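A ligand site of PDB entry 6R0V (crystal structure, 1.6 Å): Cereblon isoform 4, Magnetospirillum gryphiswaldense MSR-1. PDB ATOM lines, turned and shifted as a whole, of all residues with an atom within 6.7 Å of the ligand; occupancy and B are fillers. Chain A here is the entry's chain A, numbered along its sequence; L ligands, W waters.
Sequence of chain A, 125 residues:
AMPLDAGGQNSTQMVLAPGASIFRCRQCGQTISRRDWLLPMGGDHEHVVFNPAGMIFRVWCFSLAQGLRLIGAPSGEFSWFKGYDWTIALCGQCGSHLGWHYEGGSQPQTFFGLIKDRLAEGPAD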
ATOM      1  N   VAL A  49     -26.309  29.716  -6.737  1.00  0.00           N
ATOM      2  CA  VAL A  49     -26.964  28.852  -5.769  1.00  0.00           C
ATOM      3  C   VAL A  49     -27.101  29.521  -4.416  1.00  0.00           C
ATOM      4  O   VAL A  49     -26.448  30.534  -4.191  1.00  0.00           O
ATOM      5  CB  VAL A  49     -26.161  27.534  -5.599  1.00  0.00           C
ATOM      6  CG1 VAL A  49     -26.159  26.731  -6.915  1.00  0.00           C
ATOM      7  CG2 VAL A  49     -24.723  27.773  -5.107  1.00  0.00           C
ATOM      8  N   PHE A  50     -27.990  29.018  -3.564  1.00  0.00           N
ATOM      9  CA  PHE A  50     -28.011  29.460  -2.181  1.00  0.00           C
ATOM     10  C   PHE A  50     -28.092  28.316  -1.198  1.00  0.00           C
ATOM     11  O   PHE A  50     -28.620  27.248  -1.519  1.00  0.00           O
ATOM     12  CB  PHE A  50     -29.082  30.538  -1.920  1.00  0.00           C
ATOM     13  CG  PHE A  50     -30.453  30.029  -1.888  1.00  0.00           C
ATOM     14  CD1 PHE A  50     -31.259  29.993  -3.009  1.00  0.00           C
ATOM     15  CD2 PHE A  50     -30.995  29.605  -0.658  1.00  0.00           C
ATOM     16  CE1 PHE A  50     -32.553  29.517  -2.932  1.00  0.00           C
ATOM     17  CE2 PHE A  50     -32.292  29.136  -0.575  1.00  0.00           C
ATOM     18  CZ  PHE A  50     -33.080  29.083  -1.716  1.00  0.00           C
ATOM     19  N   ASN A  51     -27.499  28.511  -0.022  1.00  0.00           N
ATOM     20  CA  ASN A  51     -27.515  27.515   1.041  1.00  0.00           C
ATOM     21  C   ASN A  51     -28.680  27.707   2.024  1.00  0.00           C
ATOM     22  O   ASN A  51     -29.440  28.674   1.894  1.00  0.00           O
ATOM     23  CB  ASN A  51     -26.123  27.409   1.691  1.00  0.00           C
ATOM     24  CG  ASN A  51     -25.767  28.592   2.572  1.00  0.00           C
ATOM     25  OD1 ASN A  51     -26.575  29.490   2.824  1.00  0.00           O
ATOM     26  ND2 ASN A  51     -24.594  28.528   3.138  1.00  0.00           N
ATOM     27  N   PRO A  52     -28.840  26.792   3.002  1.00  0.00           N
ATOM     28  CA  PRO A  52     -30.000  26.976   3.888  1.00  0.00           C
ATOM     29  C   PRO A  52     -29.974  28.252   4.720  1.00  0.00           C
ATOM     30  O   PRO A  52     -31.054  28.742   5.116  1.00  0.00           O
ATOM     31  CB  PRO A  52     -29.962  25.751   4.808  1.00  0.00           C
ATOM     32  CG  PRO A  52     -29.262  24.716   3.998  1.00  0.00           C
ATOM     33  CD  PRO A  52     -28.284  25.433   3.092  1.00  0.00           C
ATOM     34  N   ALA A  53     -28.780  28.798   4.943  1.00  0.00           N
ATOM     35  CA  ALA A  53     -28.610  30.082   5.622  1.00  0.00           C
ATOM     36  C   ALA A  53     -28.900  31.275   4.719  1.00  0.00           C
ATOM     37  O   ALA A  53     -28.748  32.416   5.156  1.00  0.00           O
ATOM     38  CB  ALA A  53     -27.224  30.172   6.215  1.00  0.00           C
ATOM     39  N   MET A  55     -27.288  32.271   2.030  1.00  0.00           N
ATOM     40  CA  MET A  55     -26.118  32.872   1.407  1.00  0.00           C
ATOM     41  C   MET A  55     -26.145  32.467  -0.044  1.00  0.00           C
ATOM     42  O   MET A  55     -26.335  31.272  -0.358  1.00  0.00           O
ATOM     43  CB  MET A  55     -24.834  32.425   2.107  1.00  0.00           C
ATOM     44  CG  MET A  55     -24.747  32.907   3.529  1.00  0.00           C
ATOM     45  SD  MET A  55     -23.249  32.393   4.345  1.00  0.00           S
ATOM     46  CE  MET A  55     -23.638  30.764   4.973  1.00  0.00           C
ATOM     47  N   PHE A  57     -24.171  32.150  -3.650  1.00  0.00           N
ATOM     48  CA  PHE A  57     -22.813  31.950  -4.148  1.00  0.00           C
ATOM     49  C   PHE A  57     -22.870  31.836  -5.657  1.00  0.00           C
ATOM     50  O   PHE A  57     -23.748  31.161  -6.203  1.00  0.00           O
ATOM     51  CB  PHE A  57     -22.208  30.678  -3.602  1.00  0.00           C
ATOM     52  CG  PHE A  57     -22.225  30.555  -2.108  1.00  0.00           C
ATOM     53  CD1 PHE A  57     -21.209  31.078  -1.342  1.00  0.00           C
ATOM     54  CD2 PHE A  57     -23.238  29.867  -1.475  1.00  0.00           C
ATOM     55  CE1 PHE A  57     -21.217  30.939   0.049  1.00  0.00           C
ATOM     56  CE2 PHE A  57     -23.207  29.737  -0.070  1.00  0.00           C
ATOM     57  CZ  PHE A  57     -22.194  30.250   0.670  1.00  0.00           C
ATOM     58  N   SER A  75     -22.004  14.726   2.861  1.00  0.00           N
ATOM     59  CA  SER A  75     -23.434  14.790   3.069  1.00  0.00           C
ATOM     60  C   SER A  75     -24.147  15.009   1.764  1.00  0.00           C
ATOM     61  O   SER A  75     -23.691  15.814   0.945  1.00  0.00           O
ATOM     62  CB  SER A  75     -23.794  15.936   4.018  1.00  0.00           C
ATOM     63  OG  SER A  75     -25.216  15.917   4.218  1.00  0.00           O
ATOM     64  N   GLU A  77     -27.288  16.093   1.881  1.00  0.00           N
ATOM     65  CA  GLU A  77     -28.317  17.058   2.277  1.00  0.00           C
ATOM     66  C   GLU A  77     -28.103  18.393   1.546  1.00  0.00           C
ATOM     67  O   GLU A  77     -27.023  18.932   1.529  1.00  0.00           O
ATOM     68  CB  GLU A  77     -28.328  17.256   3.787  1.00  0.00           C
ATOM     69  CG  GLU A  77     -29.683  17.647   4.335  1.00  0.00           C
ATOM     70  CD  GLU A  77     -29.649  17.911   5.822  1.00  0.00           C
ATOM     71  OE1 GLU A  77     -30.749  18.003   6.429  1.00  0.00           O
ATOM     72  OE2 GLU A  77     -28.534  18.088   6.360  1.00  0.00           O
ATOM     73  N   PHE A  78     -29.175  18.902   0.946  1.00  0.00           N
ATOM     74  CA  PHE A  78     -29.193  20.190   0.250  1.00  0.00           C
ATOM     75  C   PHE A  78     -28.209  20.282  -0.927  1.00  0.00           C
ATOM     76  O   PHE A  78     -27.912  21.370  -1.341  1.00  0.00           O
ATOM     77  CB  PHE A  78     -28.928  21.355   1.203  1.00  0.00           C
ATOM     78  CG  PHE A  78     -29.665  21.296   2.508  1.00  0.00           C
ATOM     79  CD1 PHE A  78     -30.997  21.516   2.546  1.00  0.00           C
ATOM     80  CD2 PHE A  78     -28.976  21.027   3.698  1.00  0.00           C
ATOM     81  CE1 PHE A  78     -31.694  21.512   3.764  1.00  0.00           C
ATOM     82  CE2 PHE A  78     -29.662  20.999   4.900  1.00  0.00           C
ATOM     83  CZ  PHE A  78     -31.013  21.240   4.932  1.00  0.00           C
ATOM     84  N   SER A  79     -27.739  19.186  -1.477  1.00  0.00           N
ATOM     85  CA  SER A  79     -26.752  19.265  -2.519  1.00  0.00           C
ATOM     86  C   SER A  79     -27.285  19.963  -3.738  1.00  0.00           C
ATOM     87  O   SER A  79     -28.374  19.684  -4.189  1.00  0.00           O
ATOM     88  CB  SER A  79     -26.291  17.866  -2.963  1.00  0.00           C
ATOM     89  OG  SER A  79     -25.297  18.006  -3.939  1.00  0.00           O
ATOM     90  N   TRP A  80     -26.488  20.886  -4.276  1.00  0.00           N
ATOM     91  CA  TRP A  80     -26.813  21.624  -5.477  1.00  0.00           C
ATOM     92  C   TRP A  80     -26.616  20.832  -6.763  1.00  0.00           C
ATOM     93  O   TRP A  80     -27.012  21.297  -7.853  1.00  0.00           O
ATOM     94  CB  TRP A  80     -25.985  22.886  -5.537  1.00  0.00           C
ATOM     95  CG  TRP A  80     -26.248  23.848  -4.426  1.00  0.00           C
ATOM     96  CD1 TRP A  80     -27.464  24.280  -3.951  1.00  0.00           C
ATOM     97  CD2 TRP A  80     -25.252  24.530  -3.693  1.00  0.00           C
ATOM     98  NE1 TRP A  80     -27.261  25.221  -2.967  1.00  0.00           N
ATOM     99  CE2 TRP A  80     -25.910  25.383  -2.784  1.00  0.00           C
ATOM    100  CE3 TRP A  80     -23.863  24.526  -3.697  1.00  0.00           C
ATOM    101  CZ2 TRP A  80     -25.201  26.198  -1.900  1.00  0.00           C
ATOM    102  CZ3 TRP A  80     -23.184  25.342  -2.818  1.00  0.00           C
ATOM    103  CH2 TRP A  80     -23.855  26.176  -1.944  1.00  0.00           C
ATOM    104  N   PHE A  81     -25.996  19.648  -6.670  1.00  0.00           N
ATOM    105  CA  PHE A  81     -25.659  18.867  -7.835  1.00  0.00           C
ATOM    106  C   PHE A  81     -26.181  17.469  -7.609  1.00  0.00           C
ATOM    107  O   PHE A  81     -25.713  16.762  -6.705  1.00  0.00           O
ATOM    108  CB  PHE A  81     -24.162  18.886  -8.076  1.00  0.00           C
ATOM    109  CG  PHE A  81     -23.610  20.242  -8.314  1.00  0.00           C
ATOM    110  CD1 PHE A  81     -23.681  20.797  -9.582  1.00  0.00           C
ATOM    111  CD2 PHE A  81     -23.046  20.935  -7.304  1.00  0.00           C
ATOM    112  CE1 PHE A  81     -23.080  22.046  -9.841  1.00  0.00           C
ATOM    113  CE2 PHE A  81     -22.518  22.222  -7.536  1.00  0.00           C
ATOM    114  CZ  PHE A  81     -22.531  22.770  -8.810  1.00  0.00           C
ATOM    115  N   TYR A  84     -24.599  13.964  -6.053  1.00  0.00           N
ATOM    116  CA  TYR A  84     -23.329  14.229  -5.341  1.00  0.00           C
ATOM    117  C   TYR A  84     -23.521  14.575  -3.906  1.00  0.00           C
ATOM    118  O   TYR A  84     -24.513  15.224  -3.543  1.00  0.00           O
ATOM    119  CB  TYR A  84     -22.559  15.345  -5.985  1.00  0.00           C
ATOM    120  CG  TYR A  84     -22.126  15.071  -7.390  1.00  0.00           C
ATOM    121  CD1 TYR A  84     -22.946  15.391  -8.443  1.00  0.00           C
ATOM    122  CD2 TYR A  84     -20.899  14.465  -7.665  1.00  0.00           C
ATOM    123  CE1 TYR A  84     -22.559  15.204  -9.759  1.00  0.00           C
ATOM    124  CE2 TYR A  84     -20.529  14.207  -8.968  1.00  0.00           C
ATOM    125  CZ  TYR A  84     -21.379  14.569 -10.009  1.00  0.00           C
ATOM    126  OH  TYR A  84     -21.034  14.356 -11.317  1.00  0.00           O
ATOM    127  N   TRP A  86     -21.470  16.306  -0.614  1.00  0.00           N
ATOM    128  CA  TRP A  86     -20.476  17.389  -0.471  1.00  0.00           C
ATOM    129  C   TRP A  86     -19.789  17.386   0.863  1.00  0.00           C
ATOM    130  O   TRP A  86     -20.343  16.930   1.886  1.00  0.00           O
ATOM    131  CB  TRP A  86     -21.107  18.743  -0.740  1.00  0.00           C
ATOM    132  CG  TRP A  86     -22.289  19.059   0.093  1.00  0.00           C
ATOM    133  CD1 TRP A  86     -23.581  18.879  -0.267  1.00  0.00           C
ATOM    134  CD2 TRP A  86     -22.306  19.589   1.428  1.00  0.00           C
ATOM    135  NE1 TRP A  86     -24.398  19.254   0.759  1.00  0.00           N
ATOM    136  CE2 TRP A  86     -23.647  19.691   1.815  1.00  0.00           C
ATOM    137  CE3 TRP A  86     -21.312  20.000   2.337  1.00  0.00           C
ATOM    138  CZ2 TRP A  86     -24.040  20.170   3.069  1.00  0.00           C
ATOM    139  CZ3 TRP A  86     -21.686  20.462   3.573  1.00  0.00           C
ATOM    140  CH2 TRP A  86     -23.045  20.542   3.940  1.00  0.00           C
ATOM    141  N   ILE A  88     -17.309  20.397   2.980  1.00  0.00           N
ATOM    142  CA  ILE A  88     -16.760  21.768   2.981  1.00  0.00           C
ATOM    143  C   ILE A  88     -15.273  21.716   2.646  1.00  0.00           C
ATOM    144  O   ILE A  88     -14.505  20.867   3.195  1.00  0.00           O
ATOM    145  CB  ILE A  88     -17.041  22.432   4.334  1.00  0.00           C
ATOM    146  CG1 ILE A  88     -18.551  22.768   4.399  1.00  0.00           C
ATOM    147  CG2 ILE A  88     -16.163  23.673   4.564  1.00  0.00           C
ATOM    148  CD1 ILE A  88     -19.080  23.190   5.732  1.00  0.00           C
ATOM    149  N   HIS A  97     -13.129  29.604   3.832  1.00  0.00           N
ATOM    150  CA  HIS A  97     -14.032  28.661   3.198  1.00  0.00           C
ATOM    151  C   HIS A  97     -14.131  28.962   1.709  1.00  0.00           C
ATOM    152  O   HIS A  97     -14.745  29.939   1.311  1.00  0.00           O
ATOM    153  CB  HIS A  97     -15.414  28.719   3.843  1.00  0.00           C
ATOM    154  CG  HIS A  97     -16.375  27.807   3.198  1.00  0.00           C
ATOM    155  ND1 HIS A  97     -17.738  27.991   3.284  1.00  0.00           N
ATOM    156  CD2 HIS A  97     -16.189  26.693   2.436  1.00  0.00           C
ATOM    157  CE1 HIS A  97     -18.343  27.033   2.621  1.00  0.00           C
ATOM    158  NE2 HIS A  97     -17.417  26.255   2.057  1.00  0.00           N
ATOM    159  N   GLY A  99     -15.091  26.657  -0.877  1.00  0.00           N
ATOM    160  CA  GLY A  99     -16.187  25.990  -1.533  1.00  0.00           C
ATOM    161  C   GLY A  99     -16.449  24.614  -0.986  1.00  0.00           C
ATOM    162  O   GLY A  99     -16.470  24.410   0.226  1.00  0.00           O
ATOM    163  N   TRP A 100     -16.659  23.657  -1.894  1.00  0.00           N
ATOM    164  CA  TRP A 100     -17.080  22.298  -1.522  1.00  0.00           C
ATOM    165  C   TRP A 100     -16.428  21.312  -2.473  1.00  0.00           C
ATOM    166  O   TRP A 100     -16.202  21.609  -3.634  1.00  0.00           O
ATOM    167  CB  TRP A 100     -18.600  22.147  -1.541  1.00  0.00           C
ATOM    168  CG  TRP A 100     -19.327  23.163  -0.704  1.00  0.00           C
ATOM    169  CD1 TRP A 100     -19.721  23.003   0.574  1.00  0.00           C
ATOM    170  CD2 TRP A 100     -19.643  24.509  -1.075  1.00  0.00           C
ATOM    171  NE1 TRP A 100     -20.292  24.182   1.047  1.00  0.00           N
ATOM    172  CE2 TRP A 100     -20.267  25.109   0.030  1.00  0.00           C
ATOM    173  CE3 TRP A 100     -19.474  25.259  -2.244  1.00  0.00           C
ATOM    174  CZ2 TRP A 100     -20.688  26.448   0.027  1.00  0.00           C
ATOM    175  CZ3 TRP A 100     -19.907  26.615  -2.245  1.00  0.00           C
ATOM    176  CH2 TRP A 100     -20.520  27.143  -1.122  1.00  0.00           C
ATOM    177  N   TYR A 102     -17.248  17.640  -4.107  1.00  0.00           N
ATOM    178  CA  TYR A 102     -18.367  16.758  -4.437  1.00  0.00           C
ATOM    179  C   TYR A 102     -17.858  15.385  -4.791  1.00  0.00           C
ATOM    180  O   TYR A 102     -16.888  15.225  -5.507  1.00  0.00           O
ATOM    181  CB  TYR A 102     -19.162  17.377  -5.596  1.00  0.00           C
ATOM    182  CG  TYR A 102     -19.888  18.631  -5.153  1.00  0.00           C
ATOM    183  CD1 TYR A 102     -21.138  18.556  -4.546  1.00  0.00           C
ATOM    184  CD2 TYR A 102     -19.278  19.863  -5.269  1.00  0.00           C
ATOM    185  CE1 TYR A 102     -21.776  19.735  -4.102  1.00  0.00           C
ATOM    186  CE2 TYR A 102     -19.927  21.027  -4.848  1.00  0.00           C
ATOM    187  CZ  TYR A 102     -21.138  20.941  -4.235  1.00  0.00           C
ATOM    188  OH  TYR A 102     -21.761  22.090  -3.813  1.00  0.00           O
HETATM  189  C1  LIG L   1     -23.174  22.726  -0.450  1.00  0.00           C
HETATM  190  C2  LIG L   1     -22.668  25.104   4.972  1.00  0.00           C
HETATM  191  C3  LIG L   1     -23.566  24.428   4.132  1.00  0.00           C
HETATM  192  C4  LIG L   1     -24.565  23.620   4.702  1.00  0.00           C
HETATM  193  C5  LIG L   1     -23.571  24.672   2.658  1.00  0.00           C
HETATM  194  C6  LIG L   1     -22.733  24.908   6.347  1.00  0.00           C
HETATM  195  C7  LIG L   1     -23.673  24.098   6.924  1.00  0.00           C
HETATM  196  C8  LIG L   1     -24.593  23.450   6.084  1.00  0.00           C
HETATM  197  C9  LIG L   1     -21.611  25.998   4.416  1.00  0.00           C
HETATM  198  N1  LIG L   1     -25.467  22.706  -0.903  1.00  0.00           N
HETATM  199  N2  LIG L   1     -23.567  23.600   1.838  1.00  0.00           N
HETATM  200  C10 LIG L   1     -24.257  22.252  -1.369  1.00  0.00           C
HETATM  201  N3  LIG L   1     -25.597  22.574   6.672  1.00  0.00           N
HETATM  202  C11 LIG L   1     -23.870  23.763   0.435  1.00  0.00           C
HETATM  203  C12 LIG L   1     -25.343  23.557   0.172  1.00  0.00           C
HETATM  204  O1  LIG L   1     -24.136  21.600  -2.384  1.00  0.00           O
HETATM  205  O2  LIG L   1     -26.284  24.009   0.814  1.00  0.00           O
HETATM  206  O3  LIG L   1     -23.560  25.819   2.201  1.00  0.00           O
HETATM  207  O4  LIG L   1     -25.793  22.638   7.886  1.00  0.00           O
HETATM  208  O5  LIG L   1     -26.200  21.817   5.950  1.00  0.00           O
HETATM  209  O6  LIG L   1     -20.888  25.509   3.522  1.00  0.00           O
HETATM  210  O7  LIG L   1     -21.509  27.149   4.880  1.00  0.00           O
HETATM  211  O   HOH W   1     -23.924  28.128   6.203  1.00  0.00           O
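The backbone carbonyl oxygen (O) of Phe 78 sits at hydrogen-bond distance from a nitrogen (N1) of the ligand (2.8 Å).
ND2 of Asn 51 is in hydrogen-bond range of O3 of the ligand, at 3.0 Å.
O6 of the ligand sits at hydrogen-bond distance from NE1 of Trp 100 (2.9 Å).
An oxygen (O1) of the ligand is in hydrogen-bond range of the side-chain hydroxyl (OH) of Tyr 102.
N of Trp 80 is in hydrogen-bond range of O1 of the ligand, at 3.1 Å.
A ring nitrogen (NE2) of His 97 sits at hydrogen-bond distance from the backbone carbonyl oxygen (O) of Gly 99, at 2.8 Å.
The backbone NH (N) of Trp 86 is in hydrogen-bond range of the backbone carbonyl oxygen (O) of Ser 75 (2.8 Å).
OD1 of Asn 51 sits at hydrogen-bond distance from N of Met 55, 3.0 Å away.
The indole nitrogen (NE1) of Trp 80 lies within hydrogen-bond range of the backbone carbonyl oxygen (O) of Phe 50.
The indole nitrogen of Trp 86 is in hydrogen-bond range of the backbone carbonyl oxygen of Glu 77.
The backbone NH of Ala 53 lies close to the side-chain amide oxygen of Asn 51.
O of Tyr 84 is in hydrogen-bond range of OG of Ser 79.
OG of Ser 79 is in hydrogen-bond range of O of Phe 81 (3.1 Å).
Merely in contact with the ligand: Pro 52 (3.3 Å), Ser 79 (3.5 Å), Trp 86 (3.5 Å), Ile 88 (3.7 Å) and His 97 (3.1 Å).
Hydrophobic or aromatic side chains that line the ligand: Pro 52, Phe 78, Trp 80, Trp 86, Ile 88, His 97, Trp 100 and Tyr 102.
Within 4 Å of the ligand: Asn 51, Pro 52, Phe 78, Ser 79, Trp 80, Trp 86, Ile 88, His 97, Trp 100 and Tyr 102.
Water W1 lies within hydrogen-bond range of O7 of the ligand and ND2 of Asn 51.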
